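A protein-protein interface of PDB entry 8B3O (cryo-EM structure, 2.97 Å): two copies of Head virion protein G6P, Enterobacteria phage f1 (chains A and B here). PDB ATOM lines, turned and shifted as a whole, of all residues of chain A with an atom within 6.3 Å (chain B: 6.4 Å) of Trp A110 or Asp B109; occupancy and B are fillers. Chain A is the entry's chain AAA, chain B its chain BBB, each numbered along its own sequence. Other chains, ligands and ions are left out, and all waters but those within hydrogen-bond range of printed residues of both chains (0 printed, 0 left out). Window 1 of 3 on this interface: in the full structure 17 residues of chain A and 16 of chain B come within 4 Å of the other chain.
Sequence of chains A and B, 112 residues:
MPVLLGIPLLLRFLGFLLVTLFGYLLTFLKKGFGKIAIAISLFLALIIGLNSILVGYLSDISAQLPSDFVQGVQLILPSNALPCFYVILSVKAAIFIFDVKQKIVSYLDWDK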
ATOM      1  N   GLY A  32     -12.230 -11.175 -15.261  1.00  0.00           N
ATOM      2  CA  GLY A  32     -11.024 -10.590 -15.826  1.00  0.00           C
ATOM      3  C   GLY A  32     -11.016 -10.572 -17.354  1.00  0.00           C
ATOM      4  O   GLY A  32     -10.279  -9.791 -17.946  1.00  0.00           O
ATOM      5  N   LYS A  35     -12.892  -7.282 -18.300  1.00  0.00           N
ATOM      6  CA  LYS A  35     -12.085  -6.079 -18.194  1.00  0.00           C
ATOM      7  C   LYS A  35     -11.434  -5.780 -19.545  1.00  0.00           C
ATOM      8  O   LYS A  35     -11.366  -4.620 -19.949  1.00  0.00           O
ATOM      9  CB  LYS A  35     -11.064  -6.271 -17.067  1.00  0.00           C
ATOM     10  CG  LYS A  35     -10.114  -5.113 -16.794  1.00  0.00           C
ATOM     11  CD  LYS A  35      -8.695  -5.585 -16.542  1.00  0.00           C
ATOM     12  CE  LYS A  35      -8.496  -6.298 -15.220  1.00  0.00           C
ATOM     13  NZ  LYS A  35      -7.140  -6.891 -15.125  1.00  0.00           N
ATOM     14  N   ILE A  36     -10.983  -6.833 -20.244  1.00  0.00           N
ATOM     15  CA  ILE A  36     -10.333  -6.692 -21.542  1.00  0.00           C
ATOM     16  C   ILE A  36     -11.381  -6.387 -22.616  1.00  0.00           C
ATOM     17  O   ILE A  36     -11.032  -5.955 -23.711  1.00  0.00           O
ATOM     18  CB  ILE A  36      -9.445  -7.912 -21.882  1.00  0.00           C
ATOM     19  CG1 ILE A  36      -8.597  -8.358 -20.688  1.00  0.00           C
ATOM     20  CG2 ILE A  36      -8.570  -7.634 -23.102  1.00  0.00           C
ATOM     21  CD1 ILE A  36      -8.391  -9.856 -20.601  1.00  0.00           C
ATOM     22  N   ALA A  39     -11.909  -2.419 -21.821  1.00  0.00           N
ATOM     23  CA  ALA A  39     -10.698  -1.728 -22.244  1.00  0.00           C
ATOM     24  C   ALA A  39     -10.673  -1.501 -23.756  1.00  0.00           C
ATOM     25  O   ALA A  39     -10.450  -0.374 -24.194  1.00  0.00           O
ATOM     26  CB  ALA A  39      -9.477  -2.477 -21.765  1.00  0.00           C
ATOM     27  N   SER A 106      -2.113  -7.294 -29.081  1.00  0.00           N
ATOM     28  CA  SER A 106      -1.333  -7.115 -27.866  1.00  0.00           C
ATOM     29  C   SER A 106      -2.210  -7.242 -26.621  1.00  0.00           C
ATOM     30  O   SER A 106      -1.689  -7.296 -25.507  1.00  0.00           O
ATOM     31  CB  SER A 106      -0.580  -5.810 -27.892  1.00  0.00           C
ATOM     32  OG  SER A 106       0.114  -5.601 -26.671  1.00  0.00           O
ATOM     33  N   TYR A 107      -3.535  -7.300 -26.816  1.00  0.00           N
ATOM     34  CA  TYR A 107      -4.476  -7.497 -25.722  1.00  0.00           C
ATOM     35  C   TYR A 107      -4.535  -8.971 -25.325  1.00  0.00           C
ATOM     36  O   TYR A 107      -5.185  -9.319 -24.339  1.00  0.00           O
ATOM     37  CB  TYR A 107      -5.853  -6.915 -26.059  1.00  0.00           C
ATOM     38  CG  TYR A 107      -6.003  -5.436 -25.802  1.00  0.00           C
ATOM     39  CD1 TYR A 107      -6.077  -4.935 -24.508  1.00  0.00           C
ATOM     40  CD2 TYR A 107      -6.091  -4.535 -26.853  1.00  0.00           C
ATOM     41  CE1 TYR A 107      -6.215  -3.576 -24.265  1.00  0.00           C
ATOM     42  CE2 TYR A 107      -6.229  -3.173 -26.628  1.00  0.00           C
ATOM     43  CZ  TYR A 107      -6.292  -2.692 -25.330  1.00  0.00           C
ATOM     44  OH  TYR A 107      -6.430  -1.354 -25.099  1.00  0.00           O
ATOM     45  N   LEU A 108      -3.834  -9.823 -26.084  1.00  0.00           N
ATOM     46  CA  LEU A 108      -3.763 -11.250 -25.803  1.00  0.00           C
ATOM     47  C   LEU A 108      -2.786 -11.532 -24.661  1.00  0.00           C
ATOM     48  O   LEU A 108      -2.644 -12.683 -24.253  1.00  0.00           O
ATOM     49  CB  LEU A 108      -3.368 -12.009 -27.076  1.00  0.00           C
ATOM     50  CG  LEU A 108      -4.520 -12.440 -27.985  1.00  0.00           C
ATOM     51  CD1 LEU A 108      -3.992 -13.106 -29.247  1.00  0.00           C
ATOM     52  CD2 LEU A 108      -5.481 -13.376 -27.263  1.00  0.00           C
ATOM     53  N   ASP A 109      -2.134 -10.480 -24.145  1.00  0.00           N
ATOM     54  CA  ASP A 109      -1.171 -10.599 -23.059  1.00  0.00           C
ATOM     55  C   ASP A 109      -1.743 -10.005 -21.771  1.00  0.00           C
ATOM     56  O   ASP A 109      -1.045  -9.915 -20.761  1.00  0.00           O
ATOM     57  CB  ASP A 109       0.181  -9.993 -23.452  1.00  0.00           C
ATOM     58  CG  ASP A 109       1.354 -10.557 -22.666  1.00  0.00           C
ATOM     59  OD1 ASP A 109       1.403 -11.792 -22.485  1.00  0.00           O
ATOM     60  OD2 ASP A 109       2.213  -9.756 -22.240  1.00  0.00           O
ATOM     61  N   TRP A 110      -3.025  -9.623 -21.820  1.00  0.00           N
ATOM     62  CA  TRP A 110      -3.741  -9.083 -20.674  1.00  0.00           C
ATOM     63  C   TRP A 110      -4.352 -10.209 -19.839  1.00  0.00           C
ATOM     64  O   TRP A 110      -4.687 -10.001 -18.674  1.00  0.00           O
ATOM     65  CB  TRP A 110      -4.797  -8.070 -21.137  1.00  0.00           C
ATOM     66  CG  TRP A 110      -4.269  -6.695 -21.414  1.00  0.00           C
ATOM     67  CD1 TRP A 110      -3.175  -6.362 -22.162  1.00  0.00           C
ATOM     68  CD2 TRP A 110      -4.836  -5.451 -20.965  1.00  0.00           C
ATOM     69  NE1 TRP A 110      -3.015  -5.002 -22.199  1.00  0.00           N
ATOM     70  CE2 TRP A 110      -4.019  -4.417 -21.476  1.00  0.00           C
ATOM     71  CE3 TRP A 110      -5.947  -5.108 -20.181  1.00  0.00           C
ATOM     72  CZ2 TRP A 110      -4.281  -3.068 -21.226  1.00  0.00           C
ATOM     73  CZ3 TRP A 110      -6.205  -3.776 -19.934  1.00  0.00           C
ATOM     74  CH2 TRP A 110      -5.382  -2.771 -20.451  1.00  0.00           C
ATOM     75  N   ASP A 111      -4.503 -11.389 -20.455  1.00  0.00           N
ATOM     76  CA  ASP A 111      -4.958 -12.594 -19.777  1.00  0.00           C
ATOM     77  C   ASP A 111      -3.764 -13.524 -19.559  1.00  0.00           C
ATOM     78  O   ASP A 111      -3.500 -14.417 -20.365  1.00  0.00           O
ATOM     79  CB  ASP A 111      -6.164 -13.220 -20.490  1.00  0.00           C
ATOM     80  CG  ASP A 111      -6.386 -14.701 -20.221  1.00  0.00           C
ATOM     81  OD1 ASP A 111      -6.327 -15.109 -19.041  1.00  0.00           O
ATOM     82  OD2 ASP A 111      -6.643 -15.435 -21.196  1.00  0.00           O
ATOM     83  N   LYS A 112      -3.048 -13.282 -18.457  1.00  0.00           N
ATOM     84  CA  LYS A 112      -1.946 -14.126 -18.014  1.00  0.00           C
ATOM     85  C   LYS A 112      -1.877 -14.125 -16.481  1.00  0.00           C
ATOM     86  O   LYS A 112      -2.730 -13.453 -15.863  1.00  0.00           O
ATOM     87  CB  LYS A 112      -0.615 -13.713 -18.660  1.00  0.00           C
ATOM     88  CG  LYS A 112      -0.104 -12.312 -18.340  1.00  0.00           C
ATOM     89  CD  LYS A 112       1.184 -11.976 -19.060  1.00  0.00           C
ATOM     90  CE  LYS A 112       1.718 -10.606 -18.700  1.00  0.00           C
ATOM     91  NZ  LYS A 112       2.991 -10.306 -19.396  1.00  0.00           N
ATOM     92  N   VAL B 105      -6.570   4.231 -19.189  1.00  0.00           N
ATOM     93  CA  VAL B 105      -7.166   2.957 -19.574  1.00  0.00           C
ATOM     94  C   VAL B 105      -6.107   1.852 -19.521  1.00  0.00           C
ATOM     95  O   VAL B 105      -6.439   0.666 -19.552  1.00  0.00           O
ATOM     96  CB  VAL B 105      -7.865   3.056 -20.949  1.00  0.00           C
ATOM     97  CG1 VAL B 105      -8.547   1.761 -21.369  1.00  0.00           C
ATOM     98  CG2 VAL B 105      -8.868   4.198 -20.990  1.00  0.00           C
ATOM     99  N   SER B 106      -4.829   2.244 -19.423  1.00  0.00           N
ATOM    100  CA  SER B 106      -3.726   1.297 -19.346  1.00  0.00           C
ATOM    101  C   SER B 106      -3.428   0.909 -17.898  1.00  0.00           C
ATOM    102  O   SER B 106      -2.648  -0.011 -17.659  1.00  0.00           O
ATOM    103  CB  SER B 106      -2.502   1.832 -20.047  1.00  0.00           C
ATOM    104  OG  SER B 106      -1.404   0.942 -19.899  1.00  0.00           O
ATOM    105  N   TYR B 107      -4.059   1.608 -16.942  1.00  0.00           N
ATOM    106  CA  TYR B 107      -3.921   1.292 -15.528  1.00  0.00           C
ATOM    107  C   TYR B 107      -4.809   0.103 -15.156  1.00  0.00           C
ATOM    108  O   TYR B 107      -4.741  -0.390 -14.030  1.00  0.00           O
ATOM    109  CB  TYR B 107      -4.180   2.523 -14.653  1.00  0.00           C
ATOM    110  CG  TYR B 107      -2.992   3.435 -14.469  1.00  0.00           C
ATOM    111  CD1 TYR B 107      -1.913   3.061 -13.677  1.00  0.00           C
ATOM    112  CD2 TYR B 107      -2.951   4.683 -15.073  1.00  0.00           C
ATOM    113  CE1 TYR B 107      -0.819   3.896 -13.505  1.00  0.00           C
ATOM    114  CE2 TYR B 107      -1.863   5.530 -14.913  1.00  0.00           C
ATOM    115  CZ  TYR B 107      -0.795   5.135 -14.124  1.00  0.00           C
ATOM    116  OH  TYR B 107       0.278   5.961 -13.958  1.00  0.00           O
ATOM    117  N   LEU B 108      -5.619  -0.361 -16.117  1.00  0.00           N
ATOM    118  CA  LEU B 108      -6.489  -1.510 -15.922  1.00  0.00           C
ATOM    119  C   LEU B 108      -5.701  -2.817 -16.021  1.00  0.00           C
ATOM    120  O   LEU B 108      -6.271  -3.888 -15.829  1.00  0.00           O
ATOM    121  CB  LEU B 108      -7.636  -1.468 -16.940  1.00  0.00           C
ATOM    122  CG  LEU B 108      -8.882  -0.689 -16.517  1.00  0.00           C
ATOM    123  CD1 LEU B 108      -9.904  -0.650 -17.643  1.00  0.00           C
ATOM    124  CD2 LEU B 108      -9.509  -1.281 -15.262  1.00  0.00           C
ATOM    125  N   ASP B 109      -4.394  -2.716 -16.305  1.00  0.00           N
ATOM    126  CA  ASP B 109      -3.520  -3.873 -16.433  1.00  0.00           C
ATOM    127  C   ASP B 109      -2.557  -3.947 -15.248  1.00  0.00           C
ATOM    128  O   ASP B 109      -1.665  -4.795 -15.219  1.00  0.00           O
ATOM    129  CB  ASP B 109      -2.804  -3.878 -17.788  1.00  0.00           C
ATOM    130  CG  ASP B 109      -2.354  -5.259 -18.236  1.00  0.00           C
ATOM    131  OD1 ASP B 109      -3.149  -6.213 -18.094  1.00  0.00           O
ATOM    132  OD2 ASP B 109      -1.210  -5.372 -18.722  1.00  0.00           O
ATOM    133  N   TRP B 110      -2.762  -3.059 -14.266  1.00  0.00           N
ATOM    134  CA  TRP B 110      -1.970  -3.018 -13.046  1.00  0.00           C
ATOM    135  C   TRP B 110      -2.549  -3.964 -11.995  1.00  0.00           C
ATOM    136  O   TRP B 110      -1.855  -4.337 -11.050  1.00  0.00           O
ATOM    137  CB  TRP B 110      -1.862  -1.578 -12.530  1.00  0.00           C
ATOM    138  CG  TRP B 110      -0.810  -0.747 -13.203  1.00  0.00           C
ATOM    139  CD1 TRP B 110      -0.593  -0.610 -14.544  1.00  0.00           C
ATOM    140  CD2 TRP B 110       0.163   0.094 -12.556  1.00  0.00           C
ATOM    141  NE1 TRP B 110       0.450   0.245 -14.778  1.00  0.00           N
ATOM    142  CE2 TRP B 110       0.933   0.695 -13.578  1.00  0.00           C
ATOM    143  CE3 TRP B 110       0.461   0.396 -11.220  1.00  0.00           C
ATOM    144  CZ2 TRP B 110       1.979   1.577 -13.301  1.00  0.00           C
ATOM    145  CZ3 TRP B 110       1.497   1.267 -10.948  1.00  0.00           C
ATOM    146  CH2 TRP B 110       2.243   1.848 -11.976  1.00  0.00           C
ATOM    147  N   ASP B 111      -3.827  -4.330 -12.164  1.00  0.00           N
ATOM    148  CA  ASP B 111      -4.498  -5.311 -11.324  1.00  0.00           C
ATOM    149  C   ASP B 111      -4.636  -6.619 -12.101  1.00  0.00           C
ATOM    150  O   ASP B 111      -5.659  -6.876 -12.736  1.00  0.00           O
ATOM    151  CB  ASP B 111      -5.804  -4.750 -10.742  1.00  0.00           C
ATOM    152  CG  ASP B 111      -6.827  -5.791 -10.313  1.00  0.00           C
ATOM    153  OD1 ASP B 111      -6.439  -6.770  -9.641  1.00  0.00           O
ATOM    154  OD2 ASP B 111      -8.017  -5.600 -10.634  1.00  0.00           O
ATOM    155  N   LYS B 112      -3.573  -7.430 -12.043  1.00  0.00           N
ATOM    156  CA  LYS B 112      -3.551  -8.766 -12.621  1.00  0.00           C
ATOM    157  C   LYS B 112      -2.657  -9.682 -11.774  1.00  0.00           C
ATOM    158  O   LYS B 112      -2.116  -9.189 -10.762  1.00  0.00           O
ATOM    159  CB  LYS B 112      -3.132  -8.741 -14.098  1.00  0.00           C
ATOM    160  CG  LYS B 112      -1.727  -8.233 -14.403  1.00  0.00           C
ATOM    161  CD  LYS B 112      -1.421  -8.202 -15.886  1.00  0.00           C
ATOM    162  CE  LYS B 112      -0.010  -7.743 -16.186  1.00  0.00           C
ATOM    163  NZ  LYS B 112       0.275  -7.740 -17.639  1.00  0.00           N
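NZ of Lys A35 sits close to O of Leu B108 (3.2 Å). O of Asp B111 is in hydrogen-bond range of NZ of Lys A35 (2.8 Å).
The side-chain amino group of Lys A112 lies within salt-bridge range of the side-chain carboxylate of Asp A109 (3.0 Å). The side-chain amino group (NZ) of Lys B112 lies within salt-bridge range of the side-chain carboxylate (OD2) of Asp B109 (3.0 Å).
CH2 of Trp A110 touches O of Val B105, at 3.7 Å. CD2 of Trp A110 touches OD1 of Asp B109 (3.4 Å). Lys A112 touches Lys B112 (CE to NZ, 3.4 Å).
Ser A106 touches none of the printed residues of chain B. Trp A110 touches just these residues of chain B: Val B105 (3.7 Å) and Asp B109 (3.4 Å). Printed residues of chain B within 4 Å of Lys A112: Lys B112 (3.4 Å). Tyr B107 touches none of the printed residues of chain A. Of the printed residues of chain A, Leu B108 touches Lys A35. Asp B109 touches just one residue of chain A: Trp A110. Of the printed residues of chain A, Lys B112 touches Lys A112. The nearest printed residue of chain A that does not touch Leu B108 is Trp A110 (4.04 Å).
Of the 11 printed residues of chain A, 3 touch a printed residue of chain B. Among the printed residues, 5 pairs touch across the chains. Among the printed residues, no Asp or Glu carboxylate lies within 4 Å of a Lys or Arg side-chain nitrogen of the other chain.
Trp A110 touches Asp B109, but with the chains exchanged Asp A109 does not touch Trp B110 (9.6 Å). Lys B112 touches its own counterpart, Lys A112. Positions printed for both chains: 106, 107, 108, 109, 110, 111 and 112. Of the 5 pairs that touch across the chains among the printed residues, 1 has its exchanged pair printed and touching as well.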
